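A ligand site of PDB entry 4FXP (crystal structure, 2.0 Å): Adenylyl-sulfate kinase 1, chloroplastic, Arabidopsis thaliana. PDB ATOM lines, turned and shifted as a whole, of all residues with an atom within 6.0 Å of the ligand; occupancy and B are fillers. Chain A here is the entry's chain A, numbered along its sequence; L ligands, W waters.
The side-chain carboxylate of Asp 62 lies within hydrogen-bond range of an oxygen (O9) of the ligand (2.8 Å).
ND2 of Asn 82 lies within hydrogen-bond range of O4 of the ligand (2.8 Å).
An oxygen (O4) of the ligand is in salt-bridge range of the guanidinium group (NE) of Arg 65 (2.8 Å).
An oxygen (O2) of the ligand is in salt-bridge range of the guanidinium group (NH1) of Arg 79 (2.8 Å).
The backbone NH of Ser 106 sits at hydrogen-bond distance from an oxygen (O3) of the ligand (2.9 Å).
The backbone NH (N) of Ile 105 lies within hydrogen-bond range of an oxygen (O5) of the ligand (3.0 Å).
The backbone carbonyl oxygen of Gly 155 lies within hydrogen-bond range of a nitrogen (N3) of the ligand.
The side-chain carboxylate (OD1) of Asp 62 lies within salt-bridge range of the side-chain amino group (NZ) of Lys 142 (3.7 Å).
OD2 of Asp 60 lies within hydrogen-bond range of N of Asp 62 (3.0 Å).
The backbone carbonyl oxygen (O) of Ser 73 is in hydrogen-bond range of the guanidinium group (NH1) of Arg 65 (3.3 Å).
NE of Arg 79 is in hydrogen-bond range of O of Phe 74 (3.1 Å).
The guanidinium group (NH2) of Arg 79 sits at hydrogen-bond distance from the backbone carbonyl oxygen (O) of Gly 155, 3.2 Å away.
OG1 of Thr 157 is in hydrogen-bond range of NH1 of Arg 79, 2.8 Å away.
The backbone carbonyl oxygen (O) of Leu 104 sits at hydrogen-bond distance from the side-chain hydroxyl (OG) of Ser 106 (2.9 Å).
The backbone carbonyl oxygen (O) of Ser 103 lies within hydrogen-bond range of the backbone NH (N) of Gly 61 (2.9 Å).
Residues that only touch the ligand: Gly 61 (3.7 Å), Phe 74 (3.2 Å), Leu 104 (3.5 Å), Pro 107 (3.2 Å), Lys 142 (3.7 Å), Leu 144 (3.7 Å), Ile 153 (3.7 Å), Lys 154 (3.7 Å), Phe 156 (3.3 Å) and Thr 157 (3.7 Å).
Hydrophobic or aromatic side chains that line the ligand: Phe 74, Leu 104, Ile 105, Pro 107, Leu 144, Ile 153 and Phe 156.
Within 4 Å of the ligand: Gly 61, Asp 62, Arg 65, Phe 74, Arg 79, Asn 82, Leu 104, Ile 105, Ser 106, Pro 107, Lys 142, Leu 144, Ile 153, Lys 154, Gly 155, Phe 156 and Thr 157.
The nearest printed residue that does not touch the ligand is Ile 83 (4.4 Å).
Water W3 bridges the side-chain hydroxyl (OG) of Ser 34 (2.7 Å) and an oxygen (O9) of the ligand (2.7 Å).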
ATOM      1  N   SER A  34      10.434  25.037  -1.471  1.00  0.00           N
ATOM      2  CA  SER A  34      10.105  24.737  -0.088  1.00  0.00           C
ATOM      3  C   SER A  34      11.404  24.703   0.727  1.00  0.00           C
ATOM      4  O   SER A  34      12.410  24.137   0.279  1.00  0.00           O
ATOM      5  CB  SER A  34       9.378  23.399   0.004  1.00  0.00           C
ATOM      6  OG  SER A  34       9.151  23.024   1.351  1.00  0.00           O
ATOM      7  N   LYS A  38      11.246  31.425   2.740  1.00  0.00           N
ATOM      8  CA  LYS A  38      10.255  32.426   2.370  1.00  0.00           C
ATOM      9  C   LYS A  38       9.468  32.901   3.594  1.00  0.00           C
ATOM     10  O   LYS A  38       9.273  34.104   3.797  1.00  0.00           O
ATOM     11  CB  LYS A  38       9.266  31.858   1.338  1.00  0.00           C
ATOM     12  CG  LYS A  38       9.877  31.416   0.000  1.00  0.00           C
ATOM     13  CD  LYS A  38       8.774  31.009  -0.982  1.00  0.00           C
ATOM     14  CE  LYS A  38       7.982  29.812  -0.483  1.00  0.00           C
ATOM     15  NZ  LYS A  38       8.859  28.580  -0.422  1.00  0.00           N
ATOM     16  N   ASP A  60       0.128  33.884   2.380  1.00  0.00           N
ATOM     17  CA  ASP A  60       0.961  32.691   2.410  1.00  0.00           C
ATOM     18  C   ASP A  60       0.288  31.576   1.616  1.00  0.00           C
ATOM     19  O   ASP A  60      -0.911  31.328   1.828  1.00  0.00           O
ATOM     20  CB  ASP A  60       1.155  32.268   3.862  1.00  0.00           C
ATOM     21  CG  ASP A  60       1.856  30.930   4.006  1.00  0.00           C
ATOM     22  OD1 ASP A  60       3.105  30.906   4.018  1.00  0.00           O
ATOM     23  OD2 ASP A  60       1.151  29.906   4.124  1.00  0.00           O
ATOM     24  N   GLY A  61       1.048  30.898   0.765  1.00  0.00           N
ATOM     25  CA  GLY A  61       0.523  29.861  -0.097  1.00  0.00           C
ATOM     26  C   GLY A  61      -0.308  28.879   0.684  1.00  0.00           C
ATOM     27  O   GLY A  61      -1.462  28.634   0.347  1.00  0.00           O
ATOM     28  N   ASP A  62       0.280  28.299   1.717  1.00  0.00           N
ATOM     29  CA  ASP A  62      -0.443  27.286   2.471  1.00  0.00           C
ATOM     30  C   ASP A  62      -1.759  27.849   3.033  1.00  0.00           C
ATOM     31  O   ASP A  62      -2.809  27.248   2.851  1.00  0.00           O
ATOM     32  CB  ASP A  62       0.426  26.652   3.561  1.00  0.00           C
ATOM     33  CG  ASP A  62       1.381  25.595   3.007  1.00  0.00           C
ATOM     34  OD1 ASP A  62       2.575  25.898   2.777  1.00  0.00           O
ATOM     35  OD2 ASP A  62       0.928  24.448   2.776  1.00  0.00           O
ATOM     36  N   ARG A  65      -4.500  28.603   0.622  1.00  0.00           N
ATOM     37  CA  ARG A  65      -4.963  27.325   0.092  1.00  0.00           C
ATOM     38  C   ARG A  65      -5.974  26.609   0.987  1.00  0.00           C
ATOM     39  O   ARG A  65      -6.578  25.612   0.585  1.00  0.00           O
ATOM     40  CB  ARG A  65      -3.786  26.388  -0.196  1.00  0.00           C
ATOM     41  CG  ARG A  65      -3.143  26.624  -1.574  1.00  0.00           C
ATOM     42  CD  ARG A  65      -1.974  25.674  -1.773  1.00  0.00           C
ATOM     43  NE  ARG A  65      -1.423  25.721  -3.119  1.00  0.00           N
ATOM     44  CZ  ARG A  65      -1.943  25.073  -4.162  1.00  0.00           C
ATOM     45  NH1 ARG A  65      -3.055  24.351  -4.008  1.00  0.00           N
ATOM     46  NH2 ARG A  65      -1.385  25.161  -5.362  1.00  0.00           N
ATOM     47  N   SER A  73      -5.669  21.996  -6.426  1.00  0.00           N
ATOM     48  CA  SER A  73      -4.669  20.972  -6.165  1.00  0.00           C
ATOM     49  C   SER A  73      -3.293  21.463  -6.601  1.00  0.00           C
ATOM     50  O   SER A  73      -3.086  22.667  -6.788  1.00  0.00           O
ATOM     51  CB  SER A  73      -5.024  19.675  -6.907  1.00  0.00           C
ATOM     52  OG  SER A  73      -4.846  19.826  -8.299  1.00  0.00           O
ATOM     53  N   PHE A  74      -2.348  20.545  -6.771  1.00  0.00           N
ATOM     54  CA  PHE A  74      -1.000  20.915  -7.209  1.00  0.00           C
ATOM     55  C   PHE A  74      -0.644  20.536  -8.647  1.00  0.00           C
ATOM     56  O   PHE A  74       0.491  20.680  -9.085  1.00  0.00           O
ATOM     57  CB  PHE A  74       0.008  20.374  -6.185  1.00  0.00           C
ATOM     58  CG  PHE A  74      -0.175  20.959  -4.822  1.00  0.00           C
ATOM     59  CD1 PHE A  74       0.500  22.110  -4.446  1.00  0.00           C
ATOM     60  CD2 PHE A  74      -1.086  20.413  -3.936  1.00  0.00           C
ATOM     61  CE1 PHE A  74       0.304  22.679  -3.191  1.00  0.00           C
ATOM     62  CE2 PHE A  74      -1.295  20.974  -2.683  1.00  0.00           C
ATOM     63  CZ  PHE A  74      -0.601  22.097  -2.313  1.00  0.00           C
ATOM     64  N   ASP A  78      -3.554  23.965 -11.741  1.00  0.00           N
ATOM     65  CA  ASP A  78      -4.107  24.457 -10.477  1.00  0.00           C
ATOM     66  C   ASP A  78      -3.106  25.379  -9.788  1.00  0.00           C
ATOM     67  O   ASP A  78      -3.495  26.324  -9.114  1.00  0.00           O
ATOM     68  CB  ASP A  78      -4.500  23.308  -9.565  1.00  0.00           C
ATOM     69  CG  ASP A  78      -5.927  22.824  -9.806  1.00  0.00           C
ATOM     70  OD1 ASP A  78      -6.483  23.130 -10.891  1.00  0.00           O
ATOM     71  OD2 ASP A  78      -6.503  22.140  -8.934  1.00  0.00           O
ATOM     72  N   ARG A  79      -1.817  25.111  -9.971  1.00  0.00           N
ATOM     73  CA  ARG A  79      -0.792  26.017  -9.459  1.00  0.00           C
ATOM     74  C   ARG A  79      -0.875  27.352 -10.205  1.00  0.00           C
ATOM     75  O   ARG A  79      -0.727  28.410  -9.602  1.00  0.00           O
ATOM     76  CB  ARG A  79       0.617  25.432  -9.612  1.00  0.00           C
ATOM     77  CG  ARG A  79       0.920  24.207  -8.737  1.00  0.00           C
ATOM     78  CD  ARG A  79       2.425  23.972  -8.690  1.00  0.00           C
ATOM     79  NE  ARG A  79       2.812  22.612  -8.307  1.00  0.00           N
ATOM     80  CZ  ARG A  79       3.575  22.322  -7.271  1.00  0.00           C
ATOM     81  NH1 ARG A  79       4.025  23.296  -6.480  1.00  0.00           N
ATOM     82  NH2 ARG A  79       3.908  21.059  -7.004  1.00  0.00           N
ATOM     83  N   ASN A  82      -3.812  29.084  -8.722  1.00  0.00           N
ATOM     84  CA  ASN A  82      -3.403  29.495  -7.375  1.00  0.00           C
ATOM     85  C   ASN A  82      -2.637  30.820  -7.451  1.00  0.00           C
ATOM     86  O   ASN A  82      -2.964  31.782  -6.758  1.00  0.00           O
ATOM     87  CB  ASN A  82      -2.496  28.424  -6.756  1.00  0.00           C
ATOM     88  CG  ASN A  82      -2.116  28.730  -5.311  1.00  0.00           C
ATOM     89  OD1 ASN A  82      -2.964  29.051  -4.486  1.00  0.00           O
ATOM     90  ND2 ASN A  82      -0.826  28.624  -5.009  1.00  0.00           N
ATOM     91  N   ILE A  83      -1.610  30.845  -8.295  1.00  0.00           N
ATOM     92  CA  ILE A  83      -0.784  32.033  -8.477  1.00  0.00           C
ATOM     93  C   ILE A  83      -1.568  33.215  -9.041  1.00  0.00           C
ATOM     94  O   ILE A  83      -1.397  34.352  -8.601  1.00  0.00           O
ATOM     95  CB  ILE A  83       0.405  31.736  -9.422  1.00  0.00           C
ATOM     96  CG1 ILE A  83       1.362  30.725  -8.768  1.00  0.00           C
ATOM     97  CG2 ILE A  83       1.121  33.031  -9.775  1.00  0.00           C
ATOM     98  CD1 ILE A  83       2.190  29.912  -9.781  1.00  0.00           C
ATOM     99  N   SER A 103       3.807  35.068  -0.332  1.00  0.00           N
ATOM    100  CA  SER A 103       4.857  34.083  -0.110  1.00  0.00           C
ATOM    101  C   SER A 103       4.344  32.721  -0.543  1.00  0.00           C
ATOM    102  O   SER A 103       3.618  32.062   0.198  1.00  0.00           O
ATOM    103  CB  SER A 103       5.260  34.094   1.365  1.00  0.00           C
ATOM    104  OG  SER A 103       6.265  33.142   1.634  1.00  0.00           O
ATOM    105  N   LEU A 104       4.681  32.339  -1.765  1.00  0.00           N
ATOM    106  CA  LEU A 104       4.201  31.097  -2.368  1.00  0.00           C
ATOM    107  C   LEU A 104       5.381  30.506  -3.100  1.00  0.00           C
ATOM    108  O   LEU A 104       6.230  31.244  -3.577  1.00  0.00           O
ATOM    109  CB  LEU A 104       3.140  31.401  -3.419  1.00  0.00           C
ATOM    110  CG  LEU A 104       1.668  31.608  -3.124  1.00  0.00           C
ATOM    111  CD1 LEU A 104       1.450  32.789  -2.187  1.00  0.00           C
ATOM    112  CD2 LEU A 104       0.958  31.824  -4.444  1.00  0.00           C
ATOM    113  N   ILE A 105       5.413  29.181  -3.241  1.00  0.00           N
ATOM    114  CA  ILE A 105       6.474  28.579  -4.023  1.00  0.00           C
ATOM    115  C   ILE A 105       6.486  29.213  -5.418  1.00  0.00           C
ATOM    116  O   ILE A 105       7.551  29.586  -5.915  1.00  0.00           O
ATOM    117  CB  ILE A 105       6.286  27.047  -4.101  1.00  0.00           C
ATOM    118  CG1 ILE A 105       6.489  26.420  -2.712  1.00  0.00           C
ATOM    119  CG2 ILE A 105       7.247  26.432  -5.125  1.00  0.00           C
ATOM    120  CD1 ILE A 105       6.289  24.913  -2.664  1.00  0.00           C
ATOM    121  N   SER A 106       5.319  29.342  -6.027  1.00  0.00           N
ATOM    122  CA  SER A 106       5.123  30.022  -7.300  1.00  0.00           C
ATOM    123  C   SER A 106       6.171  29.634  -8.318  1.00  0.00           C
ATOM    124  O   SER A 106       6.909  30.455  -8.732  1.00  0.00           O
ATOM    125  CB  SER A 106       4.998  31.542  -7.114  1.00  0.00           C
ATOM    126  OG  SER A 106       6.004  32.054  -6.324  1.00  0.00           O
ATOM    127  N   PRO A 107       6.259  28.348  -8.669  1.00  0.00           N
ATOM    128  CA  PRO A 107       7.386  27.811  -9.430  1.00  0.00           C
ATOM    129  C   PRO A 107       7.498  28.190 -10.899  1.00  0.00           C
ATOM    130  O   PRO A 107       8.576  28.024 -11.472  1.00  0.00           O
ATOM    131  CB  PRO A 107       7.166  26.297  -9.297  1.00  0.00           C
ATOM    132  CG  PRO A 107       5.677  26.161  -9.196  1.00  0.00           C
ATOM    133  CD  PRO A 107       5.199  27.369  -8.446  1.00  0.00           C
ATOM    134  N   LYS A 142       9.583  21.159   7.556  1.00  0.00           N
ATOM    135  CA  LYS A 142       8.256  20.584   7.673  1.00  0.00           C
ATOM    136  C   LYS A 142       8.209  19.115   7.247  1.00  0.00           C
ATOM    137  O   LYS A 142       7.126  18.522   7.171  1.00  0.00           O
ATOM    138  CB  LYS A 142       7.243  21.413   6.872  1.00  0.00           C
ATOM    139  CG  LYS A 142       7.074  22.836   7.407  1.00  0.00           C
ATOM    140  CD  LYS A 142       6.153  23.664   6.515  1.00  0.00           C
ATOM    141  CE  LYS A 142       4.775  23.026   6.381  1.00  0.00           C
ATOM    142  NZ  LYS A 142       3.872  23.797   5.486  1.00  0.00           N
ATOM    143  N   LEU A 144       8.593  17.792   4.471  1.00  0.00           N
ATOM    144  CA  LEU A 144       8.070  17.586   3.116  1.00  0.00           C
ATOM    145  C   LEU A 144       9.009  16.829   2.183  1.00  0.00           C
ATOM    146  O   LEU A 144       8.571  15.958   1.439  1.00  0.00           O
ATOM    147  CB  LEU A 144       7.691  18.932   2.493  1.00  0.00           C
ATOM    148  CG  LEU A 144       6.487  19.596   3.161  1.00  0.00           C
ATOM    149  CD1 LEU A 144       6.359  21.067   2.768  1.00  0.00           C
ATOM    150  CD2 LEU A 144       5.233  18.825   2.817  1.00  0.00           C
ATOM    151  N   ILE A 153       4.465  12.074  -1.490  1.00  0.00           N
ATOM    152  CA  ILE A 153       4.028  13.207  -2.287  1.00  0.00           C
ATOM    153  C   ILE A 153       4.603  13.135  -3.695  1.00  0.00           C
ATOM    154  O   ILE A 153       5.807  13.271  -3.884  1.00  0.00           O
ATOM    155  CB  ILE A 153       4.468  14.536  -1.659  1.00  0.00           C
ATOM    156  CG1 ILE A 153       4.023  14.612  -0.198  1.00  0.00           C
ATOM    157  CG2 ILE A 153       3.920  15.718  -2.467  1.00  0.00           C
ATOM    158  CD1 ILE A 153       4.457  15.877   0.499  1.00  0.00           C
ATOM    159  N   LYS A 154       3.735  12.933  -4.677  1.00  0.00           N
ATOM    160  CA  LYS A 154       4.152  12.926  -6.078  1.00  0.00           C
ATOM    161  C   LYS A 154       4.182  14.346  -6.663  1.00  0.00           C
ATOM    162  O   LYS A 154       3.410  15.213  -6.253  1.00  0.00           O
ATOM    163  CB  LYS A 154       3.236  12.029  -6.905  1.00  0.00           C
ATOM    164  CG  LYS A 154       3.265  10.569  -6.464  1.00  0.00           C
ATOM    165  CD  LYS A 154       2.300   9.721  -7.282  1.00  0.00           C
ATOM    166  CE  LYS A 154       2.280   8.281  -6.777  1.00  0.00           C
ATOM    167  NZ  LYS A 154       1.340   7.423  -7.558  1.00  0.00           N
ATOM    168  N   GLY A 155       5.066  14.582  -7.611  1.00  0.00           N
ATOM    169  CA  GLY A 155       5.173  15.884  -8.233  1.00  0.00           C
ATOM    170  C   GLY A 155       5.527  17.008  -7.269  1.00  0.00           C
ATOM    171  O   GLY A 155       4.981  18.102  -7.356  1.00  0.00           O
ATOM    172  N   PHE A 156       6.431  16.737  -6.339  1.00  0.00           N
ATOM    173  CA  PHE A 156       6.875  17.765  -5.411  1.00  0.00           C
ATOM    174  C   PHE A 156       7.902  18.678  -6.076  1.00  0.00           C
ATOM    175  O   PHE A 156       8.906  18.210  -6.616  1.00  0.00           O
ATOM    176  CB  PHE A 156       7.461  17.147  -4.144  1.00  0.00           C
ATOM    177  CG  PHE A 156       7.675  18.142  -3.034  1.00  0.00           C
ATOM    178  CD1 PHE A 156       6.591  18.686  -2.352  1.00  0.00           C
ATOM    179  CD2 PHE A 156       8.950  18.544  -2.683  1.00  0.00           C
ATOM    180  CE1 PHE A 156       6.786  19.602  -1.335  1.00  0.00           C
ATOM    181  CE2 PHE A 156       9.154  19.460  -1.670  1.00  0.00           C
ATOM    182  CZ  PHE A 156       8.068  19.997  -0.994  1.00  0.00           C
ATOM    183  N   THR A 157       7.618  19.980  -6.044  1.00  0.00           N
ATOM    184  CA  THR A 157       8.530  20.989  -6.577  1.00  0.00           C
ATOM    185  C   THR A 157       9.991  20.741  -6.188  1.00  0.00           C
ATOM    186  O   THR A 157      10.302  20.628  -5.003  1.00  0.00           O
ATOM    187  CB  THR A 157       8.141  22.377  -6.048  1.00  0.00           C
ATOM    188  OG1 THR A 157       6.777  22.657  -6.388  1.00  0.00           O
ATOM    189  CG2 THR A 157       9.043  23.445  -6.635  1.00  0.00           C
HETATM  190  S1  LIG L   1       2.367  26.772  -5.390  1.00  0.00           S
HETATM  191  O1  LIG L   1       1.032  26.564  -5.878  1.00  0.00           O
HETATM  192  O2  LIG L   1       3.317  26.029  -6.245  1.00  0.00           O
HETATM  193  O3  LIG L   1       2.678  28.216  -5.425  1.00  0.00           O
HETATM  194  P1  LIG L   1       1.988  26.865  -2.644  1.00  0.00           P
HETATM  195  O4  LIG L   1       0.678  27.548  -2.917  1.00  0.00           O
HETATM  196  O5  LIG L   1       3.028  27.812  -2.073  1.00  0.00           O
HETATM  197  O6  LIG L   1       2.497  26.209  -3.999  1.00  0.00           O
HETATM  198  O7  LIG L   1       1.776  25.658  -1.656  1.00  0.00           O
HETATM  199  C1  LIG L   1       2.858  24.941  -1.117  1.00  0.00           C
HETATM  200  C2  LIG L   1       2.568  24.118   0.040  1.00  0.00           C
HETATM  201  O8  LIG L   1       1.646  23.102  -0.343  1.00  0.00           O
HETATM  202  C3  LIG L   1       3.773  23.399   0.560  1.00  0.00           C
HETATM  203  O9  LIG L   1       4.301  24.053   1.676  1.00  0.00           O
HETATM  204  C4  LIG L   1       3.274  22.153   0.987  1.00  0.00           C
HETATM  205  O10 LIG L   1       2.839  22.281   2.309  1.00  0.00           O
HETATM  206  C5  LIG L   1       2.050  21.876   0.198  1.00  0.00           C
HETATM  207  N1  LIG L   1       2.199  20.874  -0.817  1.00  0.00           N
HETATM  208  C6  LIG L   1       1.399  19.798  -0.978  1.00  0.00           C
HETATM  209  N2  LIG L   1       1.753  19.169  -2.109  1.00  0.00           N
HETATM  210  C7  LIG L   1       2.778  19.848  -2.677  1.00  0.00           C
HETATM  211  C8  LIG L   1       3.549  19.669  -3.835  1.00  0.00           C
HETATM  212  N3  LIG L   1       3.254  18.574  -4.711  1.00  0.00           N
HETATM  213  N4  LIG L   1       4.541  20.549  -4.137  1.00  0.00           N
HETATM  214  C9  LIG L   1       4.799  21.583  -3.317  1.00  0.00           C
HETATM  215  N5  LIG L   1       4.067  21.794  -2.200  1.00  0.00           N
HETATM  216  C10 LIG L   1       3.064  20.947  -1.851  1.00  0.00           C
HETATM  217  O   HOH W   1       0.045  16.894  -2.967  1.00  0.00           O
HETATM  218  O   HOH W   2       4.227  28.155   0.249  1.00  0.00           O
HETATM  219  O   HOH W   3       6.974  24.431   1.954  1.00  0.00           O
